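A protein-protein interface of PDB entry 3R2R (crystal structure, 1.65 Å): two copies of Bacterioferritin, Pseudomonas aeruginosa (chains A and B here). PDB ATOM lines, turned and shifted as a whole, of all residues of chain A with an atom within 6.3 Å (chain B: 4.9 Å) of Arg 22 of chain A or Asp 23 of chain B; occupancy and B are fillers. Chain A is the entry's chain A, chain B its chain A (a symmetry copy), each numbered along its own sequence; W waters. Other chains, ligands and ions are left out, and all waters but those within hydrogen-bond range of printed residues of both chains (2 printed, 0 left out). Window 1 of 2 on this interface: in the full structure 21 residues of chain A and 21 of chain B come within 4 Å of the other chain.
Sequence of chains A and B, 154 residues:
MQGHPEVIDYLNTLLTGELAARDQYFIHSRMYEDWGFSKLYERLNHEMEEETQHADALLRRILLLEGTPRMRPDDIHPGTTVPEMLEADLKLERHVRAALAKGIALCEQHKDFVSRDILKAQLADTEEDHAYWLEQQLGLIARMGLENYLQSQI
NH1 of Arg 22 of chain A lies within salt-bridge range of OD1 of Asp 23 of chain B.
The guanidinium group (NH1) of Arg 22 of chain B is in salt-bridge range of the side-chain carboxylate (OD1) of Asp 23 of chain A, at 2.7 Å.
The guanidinium group (NH2) of Arg 22 of chain A lies close to the guanidinium group (NH2) of Arg 22 of chain B (3.0 Å).
Of the 21 printed residues of chain A, 7 touch a printed residue of chain B.
Hydrophobic or aromatic side chains of chain A that line the printed part of chain B: Leu 19, Phe 26, Met 71 and Pro 73.
Along chain A the printed residues that touch a printed residue of chain B span positions 19 to 73.
Of the 11 printed residues of chain B, 7 touch a printed residue of chain A.
Along chain B the printed residues that touch a printed residue of chain A span positions 19 to 76.
Among the printed residues, Asp or Glu carboxylates within 4 Å of a Lys or Arg side-chain nitrogen of the other chain: Arg 22 of chain A with Asp 23 of chain B (2.7 Å) and Asp 23 of chain A with Arg 22 of chain B (2.7 Å).
Water W1 lies within hydrogen-bond range of O of Met 71 of chain A (2.7 Å) and OD2 of Asp 23 of chain B (2.7 Å).
Water W2 lies within hydrogen-bond range of NH1 of Arg 22 of chain B (2.9 Å) and SD of Met 48 of chain A (3.7 Å).
Of the printed residues of chain B, Arg 22 of chain A touches Arg 22 (3.0 Å), Asp 23 (2.7 Å) and Phe 26 (3.9 Å).
Asp 23 of chain B touches just these residues of chain A: Arg 22 and Met 71.
Printed residues of chain A within 4 Å of Pro 73 of chain B: Pro 73 (3.8 Å).
Of the printed residues of chain A, Ile 27 of chain B touches Met 71.
Printed residues of chain B within 4 Å of Met 71 of chain A: Asp 23, Ile 27 and Ile 76.
Of the printed residues of chain B, Phe 26 of chain A touches Leu 19 and Arg 22.
The nearest printed residue of chain B that does not touch Arg 22 of chain A is Pro 73 of chain B (5.1 Å).
The nearest residue of chain A that does not touch Asp 23 of chain B is Pro 73 of chain A (4.2 Å).
The nearest printed residue of chain A that does not touch Leu 19 of chain B is Asp 23 of chain A (4.9 Å).
O of Leu 19 of chain A sits at hydrogen-bond distance from NE of Arg 22 of chain A, 3.3 Å away.
The side-chain carboxylate of Asp 23 of chain A is in salt-bridge range of the guanidinium group of Arg 22 of chain A.
O of Met 48 of chain A sits at hydrogen-bond distance from OG1 of Thr 52 of chain A (2.9 Å).
The guanidinium group (NE) of Arg 22 of chain B lies within hydrogen-bond range of the backbone carbonyl oxygen (O) of Leu 19 of chain B, at 3.3 Å.
The side-chain carboxylate (OD1) of Asp 23 of chain B lies within salt-bridge range of the guanidinium group (NE) of Arg 22 of chain B, at 3.1 Å.
Leu 19 of chain A touches Phe 26 of chain B, and with the chains exchanged Phe 26 of chain A touches Leu 19 of chain B.
Arg 22 of chain B touches its own counterpart, Arg 22 of chain A.
Arg 22 of chain A touches Asp 23 of chain B, and with the chains exchanged Asp 23 of chain A touches Arg 22 of chain B.
Pro 73 of chain A touches its own counterpart, Pro 73 of chain B.
Positions printed for both chains: 19, 20, 21, 22, 23, 24, 25, 26, 27 and 73.
Of the 12 pairs that touch across the chains among the printed residues, 8 have their exchanged pair printed and touching as well.
Among the printed residues, pairs that only touch across the chains: Met 71 of chain A with Ile 76 of chain B (3.7 Å), Met 71 of chain A with Asp 23 of chain B (3.7 Å), Pro 73 of chain A with Pro 73 of chain B (3.8 Å), Leu 19 of chain A with Phe 26 of chain B (3.8 Å), Phe 26 of chain A with Leu 19 of chain B (3.8 Å), Met 71 of chain A with Ile 27 of chain B (3.9 Å), Thr 52 of chain A with Phe 26 of chain B (3.9 Å), Arg 22 of chain A with Phe 26 of chain B (3.9 Å) and Phe 26 of chain A with Arg 22 of chain B (3.9 Å).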
ATOM      1  N   GLY A  17     -22.375  16.316  22.075  1.00  0.00           N
ATOM      2  CA  GLY A  17     -23.071  17.603  22.099  1.00  0.00           C
ATOM      3  C   GLY A  17     -24.163  17.650  21.015  1.00  0.00           C
ATOM      4  O   GLY A  17     -25.251  18.162  21.231  1.00  0.00           O
ATOM      5  N   GLU A  18     -23.881  17.127  19.828  1.00  0.00           N
ATOM      6  CA  GLU A  18     -24.887  17.166  18.749  1.00  0.00           C
ATOM      7  C   GLU A  18     -26.031  16.178  18.978  1.00  0.00           C
ATOM      8  O   GLU A  18     -27.199  16.466  18.662  1.00  0.00           O
ATOM      9  CB  GLU A  18     -24.245  16.876  17.385  1.00  0.00           C
ATOM     10  CG  GLU A  18     -23.177  17.899  17.016  1.00  0.00           C
ATOM     11  CD  GLU A  18     -23.738  19.307  16.938  1.00  0.00           C
ATOM     12  OE1 GLU A  18     -24.803  19.484  16.306  1.00  0.00           O
ATOM     13  OE2 GLU A  18     -23.077  20.215  17.490  1.00  0.00           O
ATOM     14  N   LEU A  19     -25.710  15.021  19.542  1.00  0.00           N
ATOM     15  CA  LEU A  19     -26.738  14.047  19.888  1.00  0.00           C
ATOM     16  C   LEU A  19     -27.673  14.646  20.934  1.00  0.00           C
ATOM     17  O   LEU A  19     -28.894  14.446  20.899  1.00  0.00           O
ATOM     18  CB  LEU A  19     -26.119  12.753  20.426  1.00  0.00           C
ATOM     19  CG  LEU A  19     -25.269  11.993  19.383  1.00  0.00           C
ATOM     20  CD1 LEU A  19     -24.479  10.858  20.068  1.00  0.00           C
ATOM     21  CD2 LEU A  19     -26.168  11.381  18.261  1.00  0.00           C
ATOM     22  N   ALA A  20     -27.102  15.408  21.866  1.00  0.00           N
ATOM     23  CA  ALA A  20     -27.923  16.108  22.860  1.00  0.00           C
ATOM     24  C   ALA A  20     -28.799  17.201  22.242  1.00  0.00           C
ATOM     25  O   ALA A  20     -29.981  17.326  22.598  1.00  0.00           O
ATOM     26  CB  ALA A  20     -27.004  16.740  23.919  1.00  0.00           C
ATOM     27  N   ALA A  21     -28.228  18.004  21.334  1.00  0.00           N
ATOM     28  CA  ALA A  21     -29.021  19.063  20.657  1.00  0.00           C
ATOM     29  C   ALA A  21     -30.218  18.402  19.940  1.00  0.00           C
ATOM     30  O   ALA A  21     -31.363  18.872  20.074  1.00  0.00           O
ATOM     31  CB  ALA A  21     -28.140  19.837  19.673  1.00  0.00           C
ATOM     32  N   ARG A  22     -29.964  17.294  19.214  1.00  0.00           N
ATOM     33  CA  ARG A  22     -31.044  16.527  18.559  1.00  0.00           C
ATOM     34  C   ARG A  22     -32.120  16.174  19.600  1.00  0.00           C
ATOM     35  O   ARG A  22     -33.302  16.359  19.373  1.00  0.00           O
ATOM     36  CB  ARG A  22     -30.464  15.245  17.955  1.00  0.00           C
ATOM     37  CG  ARG A  22     -31.488  14.180  17.583  1.00  0.00           C
ATOM     38  CD  ARG A  22     -30.759  12.815  17.380  1.00  0.00           C
ATOM     39  NE  ARG A  22     -30.225  12.352  18.684  1.00  0.00           N
ATOM     40  CZ  ARG A  22     -29.746  11.135  18.931  1.00  0.00           C
ATOM     41  NH1 ARG A  22     -29.712  10.200  17.979  1.00  0.00           N
ATOM     42  NH2 ARG A  22     -29.321  10.855  20.159  1.00  0.00           N
ATOM     43  N   ASP A  23     -31.707  15.629  20.738  1.00  0.00           N
ATOM     44  CA  ASP A  23     -32.688  15.175  21.728  1.00  0.00           C
ATOM     45  C   ASP A  23     -33.439  16.306  22.443  1.00  0.00           C
ATOM     46  O   ASP A  23     -34.606  16.162  22.801  1.00  0.00           O
ATOM     47  CB  ASP A  23     -32.017  14.214  22.720  1.00  0.00           C
ATOM     48  CG  ASP A  23     -31.747  12.855  22.085  1.00  0.00           C
ATOM     49  OD1 ASP A  23     -32.288  12.591  21.001  1.00  0.00           O
ATOM     50  OD2 ASP A  23     -31.018  12.050  22.658  1.00  0.00           O
ATOM     51  N   GLN A  24     -32.786  17.438  22.647  1.00  0.00           N
ATOM     52  CA  GLN A  24     -33.466  18.578  23.263  1.00  0.00           C
ATOM     53  C   GLN A  24     -34.524  19.108  22.278  1.00  0.00           C
ATOM     54  O   GLN A  24     -35.634  19.477  22.677  1.00  0.00           O
ATOM     55  CB  GLN A  24     -32.450  19.668  23.629  1.00  0.00           C
ATOM     56  CG  GLN A  24     -33.113  20.820  24.417  1.00  0.00           C
ATOM     57  CD  GLN A  24     -32.122  21.583  25.306  1.00  0.00           C
ATOM     58  OE1 GLN A  24     -31.388  20.992  26.074  1.00  0.00           O
ATOM     59  NE2 GLN A  24     -32.098  22.890  25.168  1.00  0.00           N
ATOM     60  N   TYR A  25     -34.188  19.133  20.995  1.00  0.00           N
ATOM     61  CA  TYR A  25     -35.195  19.567  20.024  1.00  0.00           C
ATOM     62  C   TYR A  25     -36.321  18.517  19.852  1.00  0.00           C
ATOM     63  O   TYR A  25     -37.489  18.860  19.558  1.00  0.00           O
ATOM     64  CB  TYR A  25     -34.527  19.861  18.676  1.00  0.00           C
ATOM     65  CG  TYR A  25     -33.664  21.101  18.734  1.00  0.00           C
ATOM     66  CD1 TYR A  25     -34.099  22.220  19.422  1.00  0.00           C
ATOM     67  CD2 TYR A  25     -32.461  21.162  18.063  1.00  0.00           C
ATOM     68  CE1 TYR A  25     -33.332  23.389  19.454  1.00  0.00           C
ATOM     69  CE2 TYR A  25     -31.665  22.320  18.106  1.00  0.00           C
ATOM     70  CZ  TYR A  25     -32.115  23.418  18.814  1.00  0.00           C
ATOM     71  OH  TYR A  25     -31.360  24.572  18.841  1.00  0.00           O
ATOM     72  N   PHE A  26     -35.998  17.236  20.034  1.00  0.00           N
ATOM     73  CA  PHE A  26     -37.028  16.185  20.026  1.00  0.00           C
ATOM     74  C   PHE A  26     -38.073  16.465  21.135  1.00  0.00           C
ATOM     75  O   PHE A  26     -39.274  16.580  20.871  1.00  0.00           O
ATOM     76  CB  PHE A  26     -36.314  14.832  20.252  1.00  0.00           C
ATOM     77  CG  PHE A  26     -37.094  13.613  19.847  1.00  0.00           C
ATOM     78  CD1 PHE A  26     -38.388  13.668  19.317  1.00  0.00           C
ATOM     79  CD2 PHE A  26     -36.491  12.349  20.016  1.00  0.00           C
ATOM     80  CE1 PHE A  26     -39.059  12.451  18.953  1.00  0.00           C
ATOM     81  CE2 PHE A  26     -37.139  11.155  19.638  1.00  0.00           C
ATOM     82  CZ  PHE A  26     -38.435  11.207  19.113  1.00  0.00           C
ATOM     83  N   ILE A  27     -37.625  16.591  22.387  1.00  0.00           N
ATOM     84  CA  ILE A  27     -38.588  16.870  23.455  1.00  0.00           C
ATOM     85  C   ILE A  27     -39.263  18.253  23.281  1.00  0.00           C
ATOM     86  O   ILE A  27     -40.480  18.361  23.397  1.00  0.00           O
ATOM     87  CB  ILE A  27     -37.982  16.691  24.888  1.00  0.00           C
ATOM     88  CG1 ILE A  27     -39.052  16.954  25.938  1.00  0.00           C
ATOM     89  CG2 ILE A  27     -36.813  17.604  25.133  1.00  0.00           C
ATOM     90  CD1 ILE A  27     -40.228  16.065  25.817  1.00  0.00           C
ATOM     91  N   GLU A  47     -35.239  21.378  13.095  1.00  0.00           N
ATOM     92  CA  GLU A  47     -33.919  21.501  13.724  1.00  0.00           C
ATOM     93  C   GLU A  47     -33.450  20.143  14.260  1.00  0.00           C
ATOM     94  O   GLU A  47     -32.263  19.845  14.226  1.00  0.00           O
ATOM     95  CB  GLU A  47     -33.959  22.482  14.897  1.00  0.00           C
ATOM     96  CG  GLU A  47     -34.687  23.784  14.598  1.00  0.00           C
ATOM     97  CD  GLU A  47     -33.918  24.695  13.705  1.00  0.00           C
ATOM     98  OE1 GLU A  47     -33.613  25.836  14.143  1.00  0.00           O
ATOM     99  OE2 GLU A  47     -33.657  24.301  12.553  1.00  0.00           O
ATOM    100  N   MET A  48     -34.364  19.347  14.824  1.00  0.00           N
ATOM    101  CA  MET A  48     -33.968  18.010  15.301  1.00  0.00           C
ATOM    102  C   MET A  48     -33.361  17.194  14.144  1.00  0.00           C
ATOM    103  O   MET A  48     -32.331  16.517  14.333  1.00  0.00           O
ATOM    104  CB  MET A  48     -35.180  17.242  15.881  1.00  0.00           C
ATOM    105  CG  MET A  48     -34.831  15.802  16.236  1.00  0.00           C
ATOM    106  SD  MET A  48     -36.260  14.851  16.820  1.00  0.00           S
ATOM    107  CE  MET A  48     -37.046  14.506  15.224  1.00  0.00           C
ATOM    108  N   GLU A  49     -33.937  17.304  12.937  1.00  0.00           N
ATOM    109  CA  GLU A  49     -33.406  16.584  11.756  1.00  0.00           C
ATOM    110  C   GLU A  49     -32.048  17.177  11.380  1.00  0.00           C
ATOM    111  O   GLU A  49     -31.129  16.448  11.023  1.00  0.00           O
ATOM    112  CB  GLU A  49     -34.412  16.670  10.589  1.00  0.00           C
ATOM    113  CG  GLU A  49     -35.708  15.975  10.960  1.00  0.00           C
ATOM    114  CD  GLU A  49     -36.801  16.128   9.888  1.00  0.00           C
ATOM    115  OE1 GLU A  49     -36.689  17.049   9.053  1.00  0.00           O
ATOM    116  OE2 GLU A  49     -37.778  15.351   9.904  1.00  0.00           O
ATOM    117  N   GLU A  51     -29.864  18.594  13.467  1.00  0.00           N
ATOM    118  CA  GLU A  51     -28.827  18.168  14.415  1.00  0.00           C
ATOM    119  C   GLU A  51     -28.493  16.692  14.187  1.00  0.00           C
ATOM    120  O   GLU A  51     -27.369  16.252  14.451  1.00  0.00           O
ATOM    121  CB  GLU A  51     -29.297  18.340  15.874  1.00  0.00           C
ATOM    122  CG  GLU A  51     -29.674  19.788  16.209  1.00  0.00           C
ATOM    123  CD  GLU A  51     -28.510  20.750  16.156  1.00  0.00           C
ATOM    124  OE1 GLU A  51     -27.430  20.385  15.742  1.00  0.00           O
ATOM    125  OE2 GLU A  51     -28.742  21.915  16.442  1.00  0.00           O
ATOM    126  N   THR A  52     -29.459  15.893  13.732  1.00  0.00           N
ATOM    127  CA  THR A  52     -29.164  14.499  13.461  1.00  0.00           C
ATOM    128  C   THR A  52     -28.144  14.436  12.321  1.00  0.00           C
ATOM    129  O   THR A  52     -27.245  13.612  12.328  1.00  0.00           O
ATOM    130  CB  THR A  52     -30.481  13.716  13.078  1.00  0.00           C
ATOM    131  OG1 THR A  52     -31.398  13.808  14.171  1.00  0.00           O
ATOM    132  CG2 THR A  52     -30.214  12.271  12.865  1.00  0.00           C
ATOM    133  N   ALA A  55     -24.741  15.428  13.773  1.00  0.00           N
ATOM    134  CA  ALA A  55     -24.181  14.292  14.473  1.00  0.00           C
ATOM    135  C   ALA A  55     -23.646  13.258  13.476  1.00  0.00           C
ATOM    136  O   ALA A  55     -22.562  12.692  13.669  1.00  0.00           O
ATOM    137  CB  ALA A  55     -25.230  13.634  15.447  1.00  0.00           C
ATOM    138  N   MET A  71     -21.382   7.496  21.831  1.00  0.00           N
ATOM    139  CA  MET A  71     -22.782   7.641  21.409  1.00  0.00           C
ATOM    140  C   MET A  71     -23.730   8.114  22.520  1.00  0.00           C
ATOM    141  O   MET A  71     -24.931   8.287  22.298  1.00  0.00           O
ATOM    142  CB  MET A  71     -23.270   6.310  20.804  1.00  0.00           C
ATOM    143  CG  MET A  71     -22.559   5.930  19.515  1.00  0.00           C
ATOM    144  SD  MET A  71     -22.806   7.174  18.183  1.00  0.00           S
ATOM    145  CE  MET A  71     -24.605   7.146  18.048  1.00  0.00           C
ATOM    146  N   ARG A  72     -23.225   8.366  23.715  1.00  0.00           N
ATOM    147  CA  ARG A  72     -24.122   8.866  24.746  1.00  0.00           C
ATOM    148  C   ARG A  72     -24.322  10.366  24.596  1.00  0.00           C
ATOM    149  O   ARG A  72     -23.364  11.146  24.660  1.00  0.00           O
ATOM    150  CB  ARG A  72     -23.564   8.547  26.143  1.00  0.00           C
ATOM    151  CG  ARG A  72     -24.654   8.437  27.155  1.00  0.00           C
ATOM    152  CD  ARG A  72     -24.098   8.137  28.512  1.00  0.00           C
ATOM    153  NE  ARG A  72     -23.213   9.213  28.913  1.00  0.00           N
ATOM    154  CZ  ARG A  72     -22.431   9.199  29.992  1.00  0.00           C
ATOM    155  NH1 ARG A  72     -22.390   8.134  30.820  1.00  0.00           N
ATOM    156  NH2 ARG A  72     -21.684  10.269  30.219  1.00  0.00           N
ATOM    157  N   PRO A  73     -25.574  10.805  24.427  1.00  0.00           N
ATOM    158  CA  PRO A  73     -25.777  12.267  24.370  1.00  0.00           C
ATOM    159  C   PRO A  73     -25.400  12.944  25.669  1.00  0.00           C
ATOM    160  O   PRO A  73     -25.600  12.311  26.736  1.00  0.00           O
ATOM    161  CB  PRO A  73     -27.306  12.417  24.153  1.00  0.00           C
ATOM    162  CG  PRO A  73     -27.756  11.070  23.643  1.00  0.00           C
ATOM    163  CD  PRO A  73     -26.818  10.031  24.198  1.00  0.00           C
ATOM    164  N   LEU A  92     -28.027  26.349  24.680  1.00  0.00           N
ATOM    165  CA  LEU A  92     -27.485  25.157  24.041  1.00  0.00           C
ATOM    166  C   LEU A  92     -26.701  25.528  22.777  1.00  0.00           C
ATOM    167  O   LEU A  92     -25.592  25.085  22.556  1.00  0.00           O
ATOM    168  CB  LEU A  92     -28.644  24.212  23.677  1.00  0.00           C
ATOM    169  CG  LEU A  92     -28.262  22.888  23.004  1.00  0.00           C
ATOM    170  CD1 LEU A  92     -27.077  22.252  23.700  1.00  0.00           C
ATOM    171  CD2 LEU A  92     -29.459  21.956  23.028  1.00  0.00           C
ATOM    172  N   LEU B  19     -34.989   5.089  22.559  1.00  0.00           N
ATOM    173  CA  LEU B  19     -33.964   6.064  22.207  1.00  0.00           C
ATOM    174  C   LEU B  19     -32.619   5.357  22.067  1.00  0.00           C
ATOM    175  O   LEU B  19     -31.817   5.667  21.177  1.00  0.00           O
ATOM    176  CB  LEU B  19     -33.861   7.168  23.264  1.00  0.00           C
ATOM    177  CG  LEU B  19     -35.133   8.039  23.374  1.00  0.00           C
ATOM    178  CD1 LEU B  19     -35.050   8.944  24.622  1.00  0.00           C
ATOM    179  CD2 LEU B  19     -35.314   8.935  22.107  1.00  0.00           C
ATOM    180  N   ALA B  20     -32.374   4.380  22.939  1.00  0.00           N
ATOM    181  CA  ALA B  20     -31.152   3.575  22.831  1.00  0.00           C
ATOM    182  C   ALA B  20     -31.126   2.705  21.571  1.00  0.00           C
ATOM    183  O   ALA B  20     -30.087   2.618  20.898  1.00  0.00           O
ATOM    184  CB  ALA B  20     -31.032   2.670  24.069  1.00  0.00           C
ATOM    185  N   ALA B  21     -32.250   2.048  21.256  1.00  0.00           N
ATOM    186  CA  ALA B  21     -32.320   1.215  20.027  1.00  0.00           C
ATOM    187  C   ALA B  21     -31.998   2.107  18.808  1.00  0.00           C
ATOM    188  O   ALA B  21     -31.179   1.723  17.952  1.00  0.00           O
ATOM    189  CB  ALA B  21     -33.702   0.574  19.900  1.00  0.00           C
ATOM    190  N   ARG B  22     -32.607   3.308  18.747  1.00  0.00           N
ATOM    191  CA  ARG B  22     -32.309   4.280  17.676  1.00  0.00           C
ATOM    192  C   ARG B  22     -30.790   4.517  17.613  1.00  0.00           C
ATOM    193  O   ARG B  22     -30.190   4.485  16.554  1.00  0.00           O
ATOM    194  CB  ARG B  22     -33.029   5.599  17.969  1.00  0.00           C
ATOM    195  CG  ARG B  22     -32.531   6.803  17.177  1.00  0.00           C
ATOM    196  CD  ARG B  22     -33.046   8.112  17.855  1.00  0.00           C
ATOM    197  NE  ARG B  22     -32.392   8.262  19.178  1.00  0.00           N
ATOM    198  CZ  ARG B  22     -32.419   9.360  19.929  1.00  0.00           C
ATOM    199  NH1 ARG B  22     -33.065  10.456  19.526  1.00  0.00           N
ATOM    200  NH2 ARG B  22     -31.766   9.357  21.086  1.00  0.00           N
ATOM    201  N   ASP B  23     -30.172   4.791  18.755  1.00  0.00           N
ATOM    202  CA  ASP B  23     -28.745   5.128  18.751  1.00  0.00           C
ATOM    203  C   ASP B  23     -27.816   3.950  18.431  1.00  0.00           C
ATOM    204  O   ASP B  23     -26.762   4.124  17.822  1.00  0.00           O
ATOM    205  CB  ASP B  23     -28.369   5.814  20.072  1.00  0.00           C
ATOM    206  CG  ASP B  23     -28.900   7.242  20.131  1.00  0.00           C
ATOM    207  OD1 ASP B  23     -29.322   7.758  19.086  1.00  0.00           O
ATOM    208  OD2 ASP B  23     -28.889   7.852  21.196  1.00  0.00           O
ATOM    209  N   GLN B  24     -28.198   2.746  18.826  1.00  0.00           N
ATOM    210  CA  GLN B  24     -27.389   1.573  18.493  1.00  0.00           C
ATOM    211  C   GLN B  24     -27.464   1.341  16.973  1.00  0.00           C
ATOM    212  O   GLN B  24     -26.463   1.000  16.333  1.00  0.00           O
ATOM    213  CB  GLN B  24     -27.888   0.347  19.269  1.00  0.00           C
ATOM    214  CG  GLN B  24     -26.965  -0.873  19.057  1.00  0.00           C
ATOM    215  CD  GLN B  24     -27.030  -1.879  20.214  1.00  0.00           C
ATOM    216  OE1 GLN B  24     -26.896  -1.516  21.367  1.00  0.00           O
ATOM    217  NE2 GLN B  24     -27.264  -3.131  19.888  1.00  0.00           N
ATOM    218  N   TYR B  25     -28.641   1.537  16.395  1.00  0.00           N
ATOM    219  CA  TYR B  25     -28.732   1.392  14.940  1.00  0.00           C
ATOM    220  C   TYR B  25     -28.020   2.550  14.199  1.00  0.00           C
ATOM    221  O   TYR B  25     -27.491   2.375  13.077  1.00  0.00           O
ATOM    222  CB  TYR B  25     -30.202   1.308  14.514  1.00  0.00           C
ATOM    223  CG  TYR B  25     -30.842   0.010  14.951  1.00  0.00           C
ATOM    224  CD1 TYR B  25     -30.141  -1.180  14.850  1.00  0.00           C
ATOM    225  CD2 TYR B  25     -32.144  -0.026  15.402  1.00  0.00           C
ATOM    226  CE1 TYR B  25     -30.729  -2.395  15.212  1.00  0.00           C
ATOM    227  CE2 TYR B  25     -32.744  -1.235  15.794  1.00  0.00           C
ATOM    228  CZ  TYR B  25     -32.016  -2.406  15.699  1.00  0.00           C
ATOM    229  OH  TYR B  25     -32.600  -3.605  16.052  1.00  0.00           O
ATOM    230  N   PHE B  26     -27.985   3.737  14.805  1.00  0.00           N
ATOM    231  CA  PHE B  26     -27.215   4.857  14.241  1.00  0.00           C
ATOM    232  C   PHE B  26     -25.722   4.459  14.121  1.00  0.00           C
ATOM    233  O   PHE B  26     -25.130   4.504  13.038  1.00  0.00           O
ATOM    234  CB  PHE B  26     -27.402   6.071  15.180  1.00  0.00           C
ATOM    235  CG  PHE B  26     -27.076   7.409  14.579  1.00  0.00           C
ATOM    236  CD1 PHE B  26     -26.615   7.573  13.268  1.00  0.00           C
ATOM    237  CD2 PHE B  26     -27.241   8.558  15.381  1.00  0.00           C
ATOM    238  CE1 PHE B  26     -26.332   8.892  12.774  1.00  0.00           C
ATOM    239  CE2 PHE B  26     -26.985   9.855  14.891  1.00  0.00           C
ATOM    240  CZ  PHE B  26     -26.518  10.021  13.582  1.00  0.00           C
ATOM    241  N   ILE B  27     -25.102   4.052  15.232  1.00  0.00           N
ATOM    242  CA  ILE B  27     -23.693   3.656  15.147  1.00  0.00           C
ATOM    243  C   ILE B  27     -23.497   2.399  14.265  1.00  0.00           C
ATOM    244  O   ILE B  27     -22.611   2.377  13.415  1.00  0.00           O
ATOM    245  CB  ILE B  27     -23.017   3.497  16.551  1.00  0.00           C
ATOM    246  CG1 ILE B  27     -21.550   3.130  16.379  1.00  0.00           C
ATOM    247  CG2 ILE B  27     -23.692   2.456  17.397  1.00  0.00           C
ATOM    248  CD1 ILE B  27     -20.780   4.126  15.601  1.00  0.00           C
ATOM    249  N   PRO B  73     -31.082   8.242  26.614  1.00  0.00           N
ATOM    250  CA  PRO B  73     -31.119   6.844  26.141  1.00  0.00           C
ATOM    251  C   PRO B  73     -30.464   5.896  27.122  1.00  0.00           C
ATOM    252  O   PRO B  73     -29.484   6.324  27.781  1.00  0.00           O
ATOM    253  CB  PRO B  73     -30.276   6.874  24.838  1.00  0.00           C
ATOM    254  CG  PRO B  73     -30.237   8.329  24.439  1.00  0.00           C
ATOM    255  CD  PRO B  73     -30.357   9.153  25.694  1.00  0.00           C
ATOM    256  N   ILE B  76     -25.881   1.731  25.338  1.00  0.00           N
ATOM    257  CA  ILE B  76     -25.888   0.787  24.229  1.00  0.00           C
ATOM    258  C   ILE B  76     -24.571   0.026  24.244  1.00  0.00           C
ATOM    259  O   ILE B  76     -23.646   0.415  24.950  1.00  0.00           O
ATOM    260  CB  ILE B  76     -26.039   1.490  22.885  1.00  0.00           C
ATOM    261  CG1 ILE B  76     -24.874   2.454  22.647  1.00  0.00           C
ATOM    262  CG2 ILE B  76     -27.444   2.173  22.806  1.00  0.00           C
ATOM    263  CD1 ILE B  76     -24.778   2.975  21.208  1.00  0.00           C
HETATM  264  O   HOH W   1     -27.046   6.783  22.848  1.00  0.00           O
HETATM  265  O   HOH W   2     -34.355  11.755  17.230  1.00  0.00           O
